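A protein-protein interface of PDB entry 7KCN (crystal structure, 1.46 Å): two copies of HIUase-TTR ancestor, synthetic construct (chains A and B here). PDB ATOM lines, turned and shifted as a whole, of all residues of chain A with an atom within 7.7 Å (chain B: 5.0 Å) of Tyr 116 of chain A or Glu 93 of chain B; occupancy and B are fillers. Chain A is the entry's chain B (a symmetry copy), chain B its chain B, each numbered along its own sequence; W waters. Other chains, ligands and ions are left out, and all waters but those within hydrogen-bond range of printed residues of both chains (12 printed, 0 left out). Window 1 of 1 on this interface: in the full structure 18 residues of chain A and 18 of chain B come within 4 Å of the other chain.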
ATOM      1  N   LEU A  17     -16.922  -1.922 -17.805  1.00  0.00           N
ATOM      2  CA  LEU A  17     -16.177  -2.320 -18.992  1.00  0.00           C
ATOM      3  C   LEU A  17     -14.995  -1.383 -19.164  1.00  0.00           C
ATOM      4  O   LEU A  17     -15.167  -0.158 -19.124  1.00  0.00           O
ATOM      5  CB  LEU A  17     -17.028  -2.249 -20.263  1.00  0.00           C
ATOM      6  CG  LEU A  17     -18.036  -3.382 -20.548  1.00  0.00           C
ATOM      7  CD1 LEU A  17     -17.381  -4.772 -20.517  1.00  0.00           C
ATOM      8  CD2 LEU A  17     -19.257  -3.239 -19.686  1.00  0.00           C
ATOM      9  N   VAL A  19     -13.173   0.061 -21.751  1.00  0.00           N
ATOM     10  CA  VAL A  19     -13.353   0.240 -23.197  1.00  0.00           C
ATOM     11  C   VAL A  19     -12.064   0.619 -23.887  1.00  0.00           C
ATOM     12  O   VAL A  19     -12.042   0.624 -25.148  1.00  0.00           O
ATOM     13  CB  VAL A  19     -14.529   1.157 -23.587  1.00  0.00           C
ATOM     14  CG1 VAL A  19     -15.827   0.598 -23.018  1.00  0.00           C
ATOM     15  CG2 VAL A  19     -14.254   2.596 -23.139  1.00  0.00           C
ATOM     16  N   LYS A  71     -26.754   5.805  -4.850  1.00  0.00           N
ATOM     17  CA  LYS A  71     -25.472   6.274  -5.378  1.00  0.00           C
ATOM     18  C   LYS A  71     -24.564   5.058  -5.523  1.00  0.00           C
ATOM     19  O   LYS A  71     -24.359   4.340  -4.530  1.00  0.00           O
ATOM     20  CB  LYS A  71     -24.856   7.270  -4.353  1.00  0.00           C
ATOM     21  CG  LYS A  71     -23.374   7.546  -4.634  1.00  0.00           C
ATOM     22  CD  LYS A  71     -22.703   8.542  -3.701  1.00  0.00           C
ATOM     23  CE  LYS A  71     -23.325   9.924  -3.707  1.00  0.00           C
ATOM     24  NZ  LYS A  71     -22.350  10.870  -3.033  1.00  0.00           N
ATOM     25  N   THR A  76     -12.185   4.460  -9.596  1.00  0.00           N
ATOM     26  CA  THR A  76     -11.641   4.391 -10.959  1.00  0.00           C
ATOM     27  C   THR A  76     -10.131   4.654 -10.996  1.00  0.00           C
ATOM     28  O   THR A  76      -9.400   3.969 -11.718  1.00  0.00           O
ATOM     29  CB  THR A  76     -12.435   5.305 -11.911  1.00  0.00           C
ATOM     30  OG1 THR A  76     -12.523   6.615 -11.319  1.00  0.00           O
ATOM     31  CG2 THR A  76     -13.860   4.827 -12.110  1.00  0.00           C
ATOM     32  N   PHE A  88      -8.024  10.381 -15.384  1.00  0.00           N
ATOM     33  CA  PHE A  88      -8.563  11.737 -15.165  1.00  0.00           C
ATOM     34  C   PHE A  88      -9.465  11.807 -13.945  1.00  0.00           C
ATOM     35  O   PHE A  88      -9.527  12.856 -13.306  1.00  0.00           O
ATOM     36  CB  PHE A  88      -9.328  12.180 -16.399  1.00  0.00           C
ATOM     37  CG  PHE A  88      -9.660  13.662 -16.466  1.00  0.00           C
ATOM     38  CD1 PHE A  88      -8.710  14.616 -16.155  1.00  0.00           C
ATOM     39  CD2 PHE A  88     -10.848  14.050 -16.989  1.00  0.00           C
ATOM     40  CE1 PHE A  88      -9.023  15.986 -16.257  1.00  0.00           C
ATOM     41  CE2 PHE A  88     -11.158  15.442 -17.116  1.00  0.00           C
ATOM     42  CZ  PHE A  88     -10.251  16.360 -16.765  1.00  0.00           C
ATOM     43  N   TYR A  89     -10.139  10.724 -13.604  1.00  0.00           N
ATOM     44  CA  TYR A  89     -11.222  10.759 -12.605  1.00  0.00           C
ATOM     45  C   TYR A  89     -10.791   9.997 -11.368  1.00  0.00           C
ATOM     46  O   TYR A  89     -10.607   8.766 -11.431  1.00  0.00           O
ATOM     47  CB  TYR A  89     -12.485  10.132 -13.173  1.00  0.00           C
ATOM     48  CG  TYR A  89     -12.833  10.677 -14.518  1.00  0.00           C
ATOM     49  CD1 TYR A  89     -13.398  11.936 -14.667  1.00  0.00           C
ATOM     50  CD2 TYR A  89     -12.609   9.909 -15.678  1.00  0.00           C
ATOM     51  CE1 TYR A  89     -13.722  12.428 -15.951  1.00  0.00           C
ATOM     52  CE2 TYR A  89     -12.932  10.413 -16.938  1.00  0.00           C
ATOM     53  CZ  TYR A  89     -13.484  11.650 -17.066  1.00  0.00           C
ATOM     54  OH  TYR A  89     -13.825  12.162 -18.293  1.00  0.00           O
ATOM     55  N   TYR A  91     -12.543   9.071  -8.890  1.00  0.00           N
ATOM     56  CA  TYR A  91     -13.635   8.114  -8.723  1.00  0.00           C
ATOM     57  C   TYR A  91     -14.787   8.574  -9.587  1.00  0.00           C
ATOM     58  O   TYR A  91     -14.769   9.692 -10.139  1.00  0.00           O
ATOM     59  CB  TYR A  91     -14.060   7.981  -7.253  1.00  0.00           C
ATOM     60  CG  TYR A  91     -14.469   9.281  -6.564  1.00  0.00           C
ATOM     61  CD1 TYR A  91     -15.734   9.811  -6.738  1.00  0.00           C
ATOM     62  CD2 TYR A  91     -13.556   9.988  -5.776  1.00  0.00           C
ATOM     63  CE1 TYR A  91     -16.110  11.010  -6.103  1.00  0.00           C
ATOM     64  CE2 TYR A  91     -13.931  11.173  -5.153  1.00  0.00           C
ATOM     65  CZ  TYR A  91     -15.196  11.666  -5.338  1.00  0.00           C
ATOM     66  OH  TYR A  91     -15.590  12.862  -4.718  1.00  0.00           O
ATOM     67  N   VAL A  92     -15.779   7.694  -9.758  1.00  0.00           N
ATOM     68  CA  VAL A  92     -16.996   8.036 -10.479  1.00  0.00           C
ATOM     69  C   VAL A  92     -18.165   7.682  -9.589  1.00  0.00           C
ATOM     70  O   VAL A  92     -18.227   6.569  -9.050  1.00  0.00           O
ATOM     71  CB  VAL A  92     -17.103   7.246 -11.793  1.00  0.00           C
ATOM     72  CG1 VAL A  92     -18.501   7.372 -12.398  1.00  0.00           C
ATOM     73  CG2 VAL A  92     -16.065   7.762 -12.769  1.00  0.00           C
ATOM     74  N   GLU A  93     -19.089   8.626  -9.428  1.00  0.00           N
ATOM     75  CA  GLU A  93     -20.358   8.379  -8.739  1.00  0.00           C
ATOM     76  C   GLU A  93     -21.526   8.543  -9.683  1.00  0.00           C
ATOM     77  O   GLU A  93     -21.560   9.470 -10.499  1.00  0.00           O
ATOM     78  CB  GLU A  93     -20.535   9.280  -7.516  1.00  0.00           C
ATOM     79  CG  GLU A  93     -19.449   9.032  -6.482  1.00  0.00           C
ATOM     80  CD  GLU A  93     -19.686   9.737  -5.157  1.00  0.00           C
ATOM     81  OE1 GLU A  93     -19.113   9.234  -4.163  1.00  0.00           O
ATOM     82  OE2 GLU A  93     -20.417  10.755  -5.150  1.00  0.00           O
ATOM     83  N   ILE A  94     -22.460   7.603  -9.604  1.00  0.00           N
ATOM     84  CA  ILE A  94     -23.666   7.652 -10.402  1.00  0.00           C
ATOM     85  C   ILE A  94     -24.806   7.694  -9.389  1.00  0.00           C
ATOM     86  O   ILE A  94     -24.958   6.759  -8.581  1.00  0.00           O
ATOM     87  CB  ILE A  94     -23.807   6.408 -11.306  1.00  0.00           C
ATOM     88  CG1 ILE A  94     -22.544   6.174 -12.128  1.00  0.00           C
ATOM     89  CG2 ILE A  94     -25.069   6.589 -12.169  1.00  0.00           C
ATOM     90  CD1 ILE A  94     -22.610   4.863 -12.982  1.00  0.00           C
ATOM     91  N   VAL A  95     -25.604   8.763  -9.431  1.00  0.00           N
ATOM     92  CA  VAL A  95     -26.690   9.028  -8.500  1.00  0.00           C
ATOM     93  C   VAL A  95     -27.981   8.886  -9.301  1.00  0.00           C
ATOM     94  O   VAL A  95     -28.130   9.504 -10.375  1.00  0.00           O
ATOM     95  CB  VAL A  95     -26.536  10.422  -7.862  1.00  0.00           C
ATOM     96  CG1 VAL A  95     -27.691  10.666  -6.904  1.00  0.00           C
ATOM     97  CG2 VAL A  95     -25.199  10.511  -7.138  1.00  0.00           C
ATOM     98  N   PRO A 108     -24.681   0.165 -15.866  1.00  0.00           N
ATOM     99  CA  PRO A 108     -23.303  -0.132 -16.296  1.00  0.00           C
ATOM    100  C   PRO A 108     -22.442   1.124 -16.337  1.00  0.00           C
ATOM    101  O   PRO A 108     -22.922   2.254 -16.322  1.00  0.00           O
ATOM    102  CB  PRO A 108     -23.423  -0.655 -17.714  1.00  0.00           C
ATOM    103  CG  PRO A 108     -24.930  -0.696 -18.049  1.00  0.00           C
ATOM    104  CD  PRO A 108     -25.625   0.142 -17.005  1.00  0.00           C
ATOM    105  N   LEU A 109     -21.133   0.884 -16.425  1.00  0.00           N
ATOM    106  CA  LEU A 109     -20.171   1.979 -16.480  1.00  0.00           C
ATOM    107  C   LEU A 109     -19.126   1.608 -17.523  1.00  0.00           C
ATOM    108  O   LEU A 109     -18.451   0.586 -17.399  1.00  0.00           O
ATOM    109  CB  LEU A 109     -19.563   2.213 -15.099  1.00  0.00           C
ATOM    110  CG  LEU A 109     -18.453   3.303 -15.006  1.00  0.00           C
ATOM    111  CD1 LEU A 109     -18.998   4.653 -15.348  1.00  0.00           C
ATOM    112  CD2 LEU A 109     -17.798   3.366 -13.609  1.00  0.00           C
ATOM    113  N   LEU A 110     -19.004   2.436 -18.564  1.00  0.00           N
ATOM    114  CA  LEU A 110     -18.042   2.206 -19.633  1.00  0.00           C
ATOM    115  C   LEU A 110     -16.895   3.149 -19.336  1.00  0.00           C
ATOM    116  O   LEU A 110     -17.116   4.362 -19.271  1.00  0.00           O
ATOM    117  CB  LEU A 110     -18.725   2.516 -20.973  1.00  0.00           C
ATOM    118  CG  LEU A 110     -20.054   1.843 -21.178  1.00  0.00           C
ATOM    119  CD1 LEU A 110     -20.499   2.202 -22.628  1.00  0.00           C
ATOM    120  CD2 LEU A 110     -19.969   0.327 -21.106  1.00  0.00           C
ATOM    121  N   LEU A 111     -15.695   2.627 -19.206  1.00  0.00           N
ATOM    122  CA  LEU A 111     -14.581   3.352 -18.640  1.00  0.00           C
ATOM    123  C   LEU A 111     -13.361   3.393 -19.567  1.00  0.00           C
ATOM    124  O   LEU A 111     -12.917   2.349 -20.080  1.00  0.00           O
ATOM    125  CB  LEU A 111     -14.234   2.643 -17.337  1.00  0.00           C
ATOM    126  CG  LEU A 111     -13.464   3.453 -16.346  1.00  0.00           C
ATOM    127  CD1 LEU A 111     -14.169   4.817 -16.049  1.00  0.00           C
ATOM    128  CD2 LEU A 111     -13.254   2.617 -15.095  1.00  0.00           C
ATOM    129  N   SER A 112     -12.765   4.578 -19.721  1.00  0.00           N
ATOM    130  CA  SER A 112     -11.390   4.657 -20.181  1.00  0.00           C
ATOM    131  C   SER A 112     -10.664   5.619 -19.248  1.00  0.00           C
ATOM    132  O   SER A 112     -11.294   6.133 -18.331  1.00  0.00           O
ATOM    133  CB  SER A 112     -11.259   5.157 -21.627  1.00  0.00           C
ATOM    134  OG  SER A 112     -11.482   6.590 -21.680  1.00  0.00           O
ATOM    135  N   ARG A 113      -9.350   5.844 -19.450  1.00  0.00           N
ATOM    136  CA  ARG A 113      -8.591   6.744 -18.560  1.00  0.00           C
ATOM    137  C   ARG A 113      -9.126   8.168 -18.635  1.00  0.00           C
ATOM    138  O   ARG A 113      -8.977   8.909 -17.652  1.00  0.00           O
ATOM    139  CB  ARG A 113      -7.122   6.720 -18.940  1.00  0.00           C
ATOM    140  CG  ARG A 113      -6.406   5.400 -18.558  1.00  0.00           C
ATOM    141  CD  ARG A 113      -5.084   5.287 -19.259  1.00  0.00           C
ATOM    142  NE  ARG A 113      -4.203   6.400 -18.813  1.00  0.00           N
ATOM    143  CZ  ARG A 113      -3.355   7.065 -19.589  1.00  0.00           C
ATOM    144  NH1 ARG A 113      -3.261   6.771 -20.884  1.00  0.00           N
ATOM    145  NH2 ARG A 113      -2.634   8.064 -19.067  1.00  0.00           N
ATOM    146  N   PHE A 114      -9.703   8.584 -19.763  1.00  0.00           N
ATOM    147  CA  PHE A 114     -10.115   9.980 -19.988  1.00  0.00           C
ATOM    148  C   PHE A 114     -11.567  10.116 -20.445  1.00  0.00           C
ATOM    149  O   PHE A 114     -11.952  11.132 -21.073  1.00  0.00           O
ATOM    150  CB  PHE A 114      -9.114  10.737 -20.910  1.00  0.00           C
ATOM    151  CG  PHE A 114      -7.819  10.868 -20.316  1.00  0.00           C
ATOM    152  CD1 PHE A 114      -7.529  11.967 -19.463  1.00  0.00           C
ATOM    153  CD2 PHE A 114      -6.845   9.909 -20.467  1.00  0.00           C
ATOM    154  CE1 PHE A 114      -6.319  12.095 -18.869  1.00  0.00           C
ATOM    155  CE2 PHE A 114      -5.627  10.014 -19.882  1.00  0.00           C
ATOM    156  CZ  PHE A 114      -5.336  11.113 -19.021  1.00  0.00           C
ATOM    157  N   SER A 115     -12.427   9.131 -20.147  1.00  0.00           N
ATOM    158  CA  SER A 115     -13.837   9.254 -20.467  1.00  0.00           C
ATOM    159  C   SER A 115     -14.612   8.200 -19.687  1.00  0.00           C
ATOM    160  O   SER A 115     -14.038   7.204 -19.234  1.00  0.00           O
ATOM    161  CB  SER A 115     -14.105   9.059 -21.986  1.00  0.00           C
ATOM    162  OG  SER A 115     -14.077   7.633 -22.341  1.00  0.00           O
ATOM    163  N   TYR A 116     -15.894   8.457 -19.480  1.00  0.00           N
ATOM    164  CA  TYR A 116     -16.792   7.399 -19.062  1.00  0.00           C
ATOM    165  C   TYR A 116     -18.217   7.698 -19.450  1.00  0.00           C
ATOM    166  O   TYR A 116     -18.576   8.840 -19.786  1.00  0.00           O
ATOM    167  CB  TYR A 116     -16.704   7.164 -17.543  1.00  0.00           C
ATOM    168  CG  TYR A 116     -17.143   8.308 -16.639  1.00  0.00           C
ATOM    169  CD1 TYR A 116     -18.465   8.375 -16.198  1.00  0.00           C
ATOM    170  CD2 TYR A 116     -16.221   9.209 -16.194  1.00  0.00           C
ATOM    171  CE1 TYR A 116     -18.890   9.357 -15.247  1.00  0.00           C
ATOM    172  CE2 TYR A 116     -16.603  10.195 -15.267  1.00  0.00           C
ATOM    173  CZ  TYR A 116     -17.948  10.245 -14.843  1.00  0.00           C
ATOM    174  OH  TYR A 116     -18.279  11.231 -13.873  1.00  0.00           O
ATOM    175  N   SER A 117     -19.041   6.655 -19.462  1.00  0.00           N
ATOM    176  CA  SER A 117     -20.436   6.821 -19.770  1.00  0.00           C
ATOM    177  C   SER A 117     -21.233   5.754 -19.062  1.00  0.00           C
ATOM    178  O   SER A 117     -20.718   4.716 -18.631  1.00  0.00           O
ATOM    179  CB  SER A 117     -20.669   6.714 -21.266  1.00  0.00           C
ATOM    180  OG  SER A 117     -19.967   5.579 -21.724  1.00  0.00           O
ATOM    181  N   THR A 118     -22.501   6.070 -18.898  1.00  0.00           N
ATOM    182  CA  THR A 118     -23.406   5.199 -18.153  1.00  0.00           C
ATOM    183  C   THR A 118     -24.789   5.353 -18.725  1.00  0.00           C
ATOM    184  O   THR A 118     -25.112   6.336 -19.395  1.00  0.00           O
ATOM    185  CB  THR A 118     -23.367   5.499 -16.641  1.00  0.00           C
ATOM    186  OG1 THR A 118     -24.105   4.468 -15.991  1.00  0.00           O
ATOM    187  CG2 THR A 118     -24.036   6.839 -16.303  1.00  0.00           C
ATOM    188  N   LYS B  71     -14.565  19.327  -8.966  1.00  0.00           N
ATOM    189  CA  LYS B  71     -15.857  18.658  -9.125  1.00  0.00           C
ATOM    190  C   LYS B  71     -16.777  19.613  -9.876  1.00  0.00           C
ATOM    191  O   LYS B  71     -16.961  20.753  -9.419  1.00  0.00           O
ATOM    192  CB  LYS B  71     -16.437  18.372  -7.710  1.00  0.00           C
ATOM    193  CG  LYS B  71     -17.924  18.000  -7.759  1.00  0.00           C
ATOM    194  CD  LYS B  71     -18.562  17.667  -6.419  1.00  0.00           C
ATOM    195  CE  LYS B  71     -17.930  16.493  -5.699  1.00  0.00           C
ATOM    196  NZ  LYS B  71     -18.879  16.064  -4.597  1.00  0.00           N
ATOM    197  N   LEU B  72     -17.407  19.162 -10.966  1.00  0.00           N
ATOM    198  CA  LEU B  72     -18.502  19.907 -11.586  1.00  0.00           C
ATOM    199  C   LEU B  72     -19.798  19.184 -11.255  1.00  0.00           C
ATOM    200  O   LEU B  72     -19.894  17.985 -11.491  1.00  0.00           O
ATOM    201  CB  LEU B  72     -18.403  19.992 -13.117  1.00  0.00           C
ATOM    202  CG  LEU B  72     -17.556  21.097 -13.690  1.00  0.00           C
ATOM    203  CD1 LEU B  72     -17.294  20.882 -15.190  1.00  0.00           C
ATOM    204  CD2 LEU B  72     -18.192  22.407 -13.458  1.00  0.00           C
ATOM    205  N   HIS B  73     -20.807  19.910 -10.831  1.00  0.00           N
ATOM    206  CA  HIS B  73     -22.080  19.346 -10.409  1.00  0.00           C
ATOM    207  C   HIS B  73     -23.162  19.979 -11.278  1.00  0.00           C
ATOM    208  O   HIS B  73     -23.329  21.206 -11.259  1.00  0.00           O
ATOM    209  CB  HIS B  73     -22.342  19.723  -8.939  1.00  0.00           C
ATOM    210  CG  HIS B  73     -23.708  19.357  -8.455  1.00  0.00           C
ATOM    211  ND1 HIS B  73     -23.907  18.361  -7.530  1.00  0.00           N
ATOM    212  CD2 HIS B  73     -24.928  19.918  -8.661  1.00  0.00           C
ATOM    213  CE1 HIS B  73     -25.198  18.274  -7.222  1.00  0.00           C
ATOM    214  NE2 HIS B  73     -25.833  19.200  -7.906  1.00  0.00           N
ATOM    215  N   PHE B  74     -23.946  19.155 -11.990  1.00  0.00           N
ATOM    216  CA  PHE B  74     -25.003  19.628 -12.886  1.00  0.00           C
ATOM    217  C   PHE B  74     -26.370  19.220 -12.384  1.00  0.00           C
ATOM    218  O   PHE B  74     -26.576  18.043 -12.077  1.00  0.00           O
ATOM    219  CB  PHE B  74     -24.803  18.985 -14.273  1.00  0.00           C
ATOM    220  CG  PHE B  74     -23.476  19.318 -14.929  1.00  0.00           C
ATOM    221  CD1 PHE B  74     -22.335  18.548 -14.677  1.00  0.00           C
ATOM    222  CD2 PHE B  74     -23.381  20.431 -15.772  1.00  0.00           C
ATOM    223  CE1 PHE B  74     -21.125  18.828 -15.319  1.00  0.00           C
ATOM    224  CE2 PHE B  74     -22.141  20.725 -16.394  1.00  0.00           C
ATOM    225  CZ  PHE B  74     -21.072  19.922 -16.183  1.00  0.00           C
ATOM    226  N   TYR B  91     -28.853  14.513 -10.239  1.00  0.00           N
ATOM    227  CA  TYR B  91     -27.764  15.401 -10.642  1.00  0.00           C
ATOM    228  C   TYR B  91     -26.632  14.541 -11.153  1.00  0.00           C
ATOM    229  O   TYR B  91     -26.656  13.301 -11.018  1.00  0.00           O
ATOM    230  CB  TYR B  91     -27.301  16.300  -9.484  1.00  0.00           C
ATOM    231  CG  TYR B  91     -26.863  15.570  -8.216  1.00  0.00           C
ATOM    232  CD1 TYR B  91     -25.600  15.019  -8.113  1.00  0.00           C
ATOM    233  CD2 TYR B  91     -27.749  15.403  -7.148  1.00  0.00           C
ATOM    234  CE1 TYR B  91     -25.197  14.346  -6.943  1.00  0.00           C
ATOM    235  CE2 TYR B  91     -27.349  14.735  -5.996  1.00  0.00           C
ATOM    236  CZ  TYR B  91     -26.086  14.210  -5.921  1.00  0.00           C
ATOM    237  OH  TYR B  91     -25.666  13.532  -4.767  1.00  0.00           O
ATOM    238  N   VAL B  92     -25.652  15.183 -11.797  1.00  0.00           N
ATOM    239  CA  VAL B  92     -24.451  14.499 -12.254  1.00  0.00           C
ATOM    240  C   VAL B  92     -23.262  15.265 -11.725  1.00  0.00           C
ATOM    241  O   VAL B  92     -23.195  16.493 -11.870  1.00  0.00           O
ATOM    242  CB  VAL B  92     -24.386  14.458 -13.789  1.00  0.00           C
ATOM    243  CG1 VAL B  92     -23.004  14.016 -14.268  1.00  0.00           C
ATOM    244  CG2 VAL B  92     -25.446  13.506 -14.307  1.00  0.00           C
ATOM    245  N   GLU B  93     -22.327  14.549 -11.106  1.00  0.00           N
ATOM    246  CA  GLU B  93     -21.042  15.117 -10.693  1.00  0.00           C
ATOM    247  C   GLU B  93     -19.899  14.463 -11.431  1.00  0.00           C
ATOM    248  O   GLU B  93     -19.879  13.242 -11.623  1.00  0.00           O
ATOM    249  CB  GLU B  93     -20.825  15.013  -9.182  1.00  0.00           C
ATOM    250  CG  GLU B  93     -21.885  15.785  -8.414  1.00  0.00           C
ATOM    251  CD  GLU B  93     -21.608  15.900  -6.925  1.00  0.00           C
ATOM    252  OE1 GLU B  93     -22.157  16.863  -6.341  1.00  0.00           O
ATOM    253  OE2 GLU B  93     -20.868  15.040  -6.392  1.00  0.00           O
ATOM    254  N   ILE B  94     -18.970  15.290 -11.894  1.00  0.00           N
ATOM    255  CA  ILE B  94     -17.786  14.811 -12.573  1.00  0.00           C
ATOM    256  C   ILE B  94     -16.618  15.311 -11.727  1.00  0.00           C
ATOM    257  O   ILE B  94     -16.452  16.532 -11.552  1.00  0.00           O
ATOM    258  CB  ILE B  94     -17.678  15.375 -14.007  1.00  0.00           C
ATOM    259  CG1 ILE B  94     -18.964  15.140 -14.792  1.00  0.00           C
ATOM    260  CG2 ILE B  94     -16.439  14.749 -14.671  1.00  0.00           C
ATOM    261  CD1 ILE B  94     -18.932  15.787 -16.217  1.00  0.00           C
ATOM    262  N   VAL B  95     -15.814  14.381 -11.209  1.00  0.00           N
ATOM    263  CA  VAL B  95     -14.701  14.648 -10.311  1.00  0.00           C
ATOM    264  C   VAL B  95     -13.433  14.328 -11.097  1.00  0.00           C
ATOM    265  O   VAL B  95     -13.308  13.229 -11.675  1.00  0.00           O
ATOM    266  CB  VAL B  95     -14.826  13.816  -9.021  1.00  0.00           C
ATOM    267  CG1 VAL B  95     -13.644  14.116  -8.112  1.00  0.00           C
ATOM    268  CG2 VAL B  95     -16.143  14.141  -8.327  1.00  0.00           C
ATOM    269  N   TYR B 116     -25.791   9.318 -19.588  1.00  0.00           N
ATOM    270  CA  TYR B 116     -24.890  10.428 -19.827  1.00  0.00           C
ATOM    271  C   TYR B 116     -23.473   9.956 -20.032  1.00  0.00           C
ATOM    272  O   TYR B 116     -23.115   8.810 -19.712  1.00  0.00           O
ATOM    273  CB  TYR B 116     -24.939  11.443 -18.670  1.00  0.00           C
ATOM    274  CG  TYR B 116     -24.467  10.960 -17.306  1.00  0.00           C
ATOM    275  CD1 TYR B 116     -23.133  11.129 -16.933  1.00  0.00           C
ATOM    276  CD2 TYR B 116     -25.370  10.446 -16.421  1.00  0.00           C
ATOM    277  CE1 TYR B 116     -22.676  10.809 -15.615  1.00  0.00           C
ATOM    278  CE2 TYR B 116     -24.955  10.109 -15.121  1.00  0.00           C
ATOM    279  CZ  TYR B 116     -23.599  10.284 -14.773  1.00  0.00           C
ATOM    280  OH  TYR B 116     -23.235   9.970 -13.433  1.00  0.00           O
ATOM    281  N   SER B 117     -22.658  10.824 -20.624  1.00  0.00           N
ATOM    282  CA  SER B 117     -21.271  10.507 -20.832  1.00  0.00           C
ATOM    283  C   SER B 117     -20.463  11.782 -20.829  1.00  0.00           C
ATOM    284  O   SER B 117     -20.975  12.892 -21.009  1.00  0.00           O
ATOM    285  CB  SER B 117     -21.078   9.792 -22.157  1.00  0.00           C
ATOM    286  OG  SER B 117     -21.802  10.509 -23.134  1.00  0.00           O
ATOM    287  N   THR B 118     -19.189  11.593 -20.555  1.00  0.00           N
ATOM    288  CA  THR B 118     -18.271  12.720 -20.419  1.00  0.00           C
ATOM    289  C   THR B 118     -16.903  12.273 -20.855  1.00  0.00           C
ATOM    290  O   THR B 118     -16.590  11.081 -20.901  1.00  0.00           O
ATOM    291  CB  THR B 118     -18.268  13.280 -18.982  1.00  0.00           C
ATOM    292  OG1 THR B 118     -17.521  14.493 -19.007  1.00  0.00           O
ATOM    293  CG2 THR B 118     -17.579  12.326 -17.995  1.00  0.00           C
HETATM  294  O   HOH W   1     -20.742  10.902 -12.618  1.00  0.00           O
HETATM  295  O   HOH W   2     -18.560  11.390  -9.766  1.00  0.00           O
HETATM  296  O   HOH W   3     -23.219  13.164  -4.252  1.00  0.00           O
HETATM  297  O   HOH W   4     -22.133  12.355  -6.954  1.00  0.00           O
HETATM  298  O   HOH W   5     -25.065  10.941 -11.305  1.00  0.00           O
HETATM  299  O   HOH W   6     -14.794  14.660 -18.388  1.00  0.00           O
HETATM  300  O   HOH W   7     -24.128   6.659 -22.143  1.00  0.00           O
HETATM  301  O   HOH W   8     -22.843  12.040  -9.893  1.00  0.00           O
HETATM  302  O   HOH W   9     -17.645   9.341 -23.019  1.00  0.00           O
HETATM  303  O   HOH W  10     -16.385  11.541 -11.606  1.00  0.00           O
HETATM  304  O   HOH W  11     -18.025  13.468  -4.415  1.00  0.00           O
HETATM  305  O   HOH W  12     -19.189  12.708  -7.099  1.00  0.00           O
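Glu 93 of chain A touches Tyr 116 of chain B, and with the chains exchanged Tyr 116 of chain A touches Glu 93 of chain B.
Tyr 116 of chain A touches Thr 118 of chain B, and with the chains exchanged Thr 118 of chain A touches Tyr 116 of chain B.
Ser 117 of chain A touches its own counterpart, Ser 117 of chain B.
Water W8 bridges the backbone NH (N) of Glu 93 of chain B and the backbone carbonyl oxygen (O) of Glu 93 of chain A.
Water W9 bridges the backbone carbonyl oxygen (O) of Thr 118 of chain B (2.9 Å) and the backbone carbonyl oxygen (O) of Tyr 116 of chain A (3.4 Å).
Water W12 lies within hydrogen-bond range of the side-chain carboxylate of Glu 93 of chain B (3.0 Å) and the side-chain carboxylate of Glu 93 of chain A (3.0 Å).
Among the printed residues, pairs that only touch across the chains: Ser 117 of chain A with Ser 117 of chain B, Tyr 89 of chain A with Val 95 of chain B, Ser 115 of chain A with Thr 118 of chain B, Tyr 116 of chain A with Ser 117 of chain B, Ser 117 of chain A with Tyr 116 of chain B, Tyr 89 of chain A with Thr 118 of chain B, Tyr 89 of chain A with Ile 94 of chain B, Val 95 of chain A with Tyr 91 of chain B, Ile 94 of chain A with Tyr 116 of chain B, Tyr 116 of chain A with Ile 94 of chain B and Tyr 91 of chain A with Val 95 of chain B.
Hydrophobic or aromatic side chains of chain B within 4 Å of the printed part of chain A: Tyr 91, Ile 94, Val 95 and Tyr 116.
Hydrophobic or aromatic side chains of chain A within 4 Å of the printed part of chain B: Tyr 89, Tyr 91, Val 95 and Tyr 116.
Among the printed residues, 15 pairs touch across the chains.
Among the printed residues, no Asp or Glu carboxylate lies within 4 Å of a Lys or Arg side-chain nitrogen of the other chain.
O of Ile 94 of chain B is in hydrogen-bond range of N of Leu 72 of chain B, at 2.9 Å.
OG of Ser 112 of chain A lies within hydrogen-bond range of OG of Ser 115 of chain A.
N of Tyr 91 of chain A lies close to OG1 of Thr 76 of chain A, 3.5 Å away.
The side-chain carboxylate (OE1) of Glu 93 of chain B is in hydrogen-bond range of a ring nitrogen (ND1) of His 73 of chain B, at 2.6 Å.
Of the printed residues of chain B, Tyr 89 of chain A touches Ile 94 (3.8 Å), Val 95 (3.3 Å) and Thr 118 (3.8 Å).
Printed residues of chain B within 4 Å of Tyr 91 of chain A: Val 95 (3.8 Å).
Printed residues of chain B within 4 Å of Val 95 of chain A: Tyr 91 (3.8 Å).
Of the printed residues of chain A, Tyr 91 of chain B touches Val 95.
Of the printed residues of chain A, Ile 94 of chain B touches Tyr 89 and Tyr 116.
The nearest printed residue of chain B that does not touch Tyr 116 of chain A is Tyr 116 of chain B (4.1 Å).
The nearest residue of chain A that does not touch Glu 93 of chain B is Glu 93 of chain A (4.3 Å).
The nearest printed residue of chain A that does not touch Thr 118 of chain B is Phe 114 of chain A (4.6 Å).
O of Tyr 116 of chain B sits at hydrogen-bond distance from N of Thr 118 of chain A (2.9 Å).
O of Glu 93 of chain B sits at hydrogen-bond distance from OH of Tyr 116 of chain A.
The backbone carbonyl oxygen (O) of Tyr 116 of chain A lies within hydrogen-bond range of the backbone NH (N) of Thr 118 of chain B (2.9 Å).
The side-chain hydroxyl (OH) of Tyr 116 of chain B is in hydrogen-bond range of the backbone carbonyl oxygen (O) of Glu 93 of chain A (3.4 Å).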
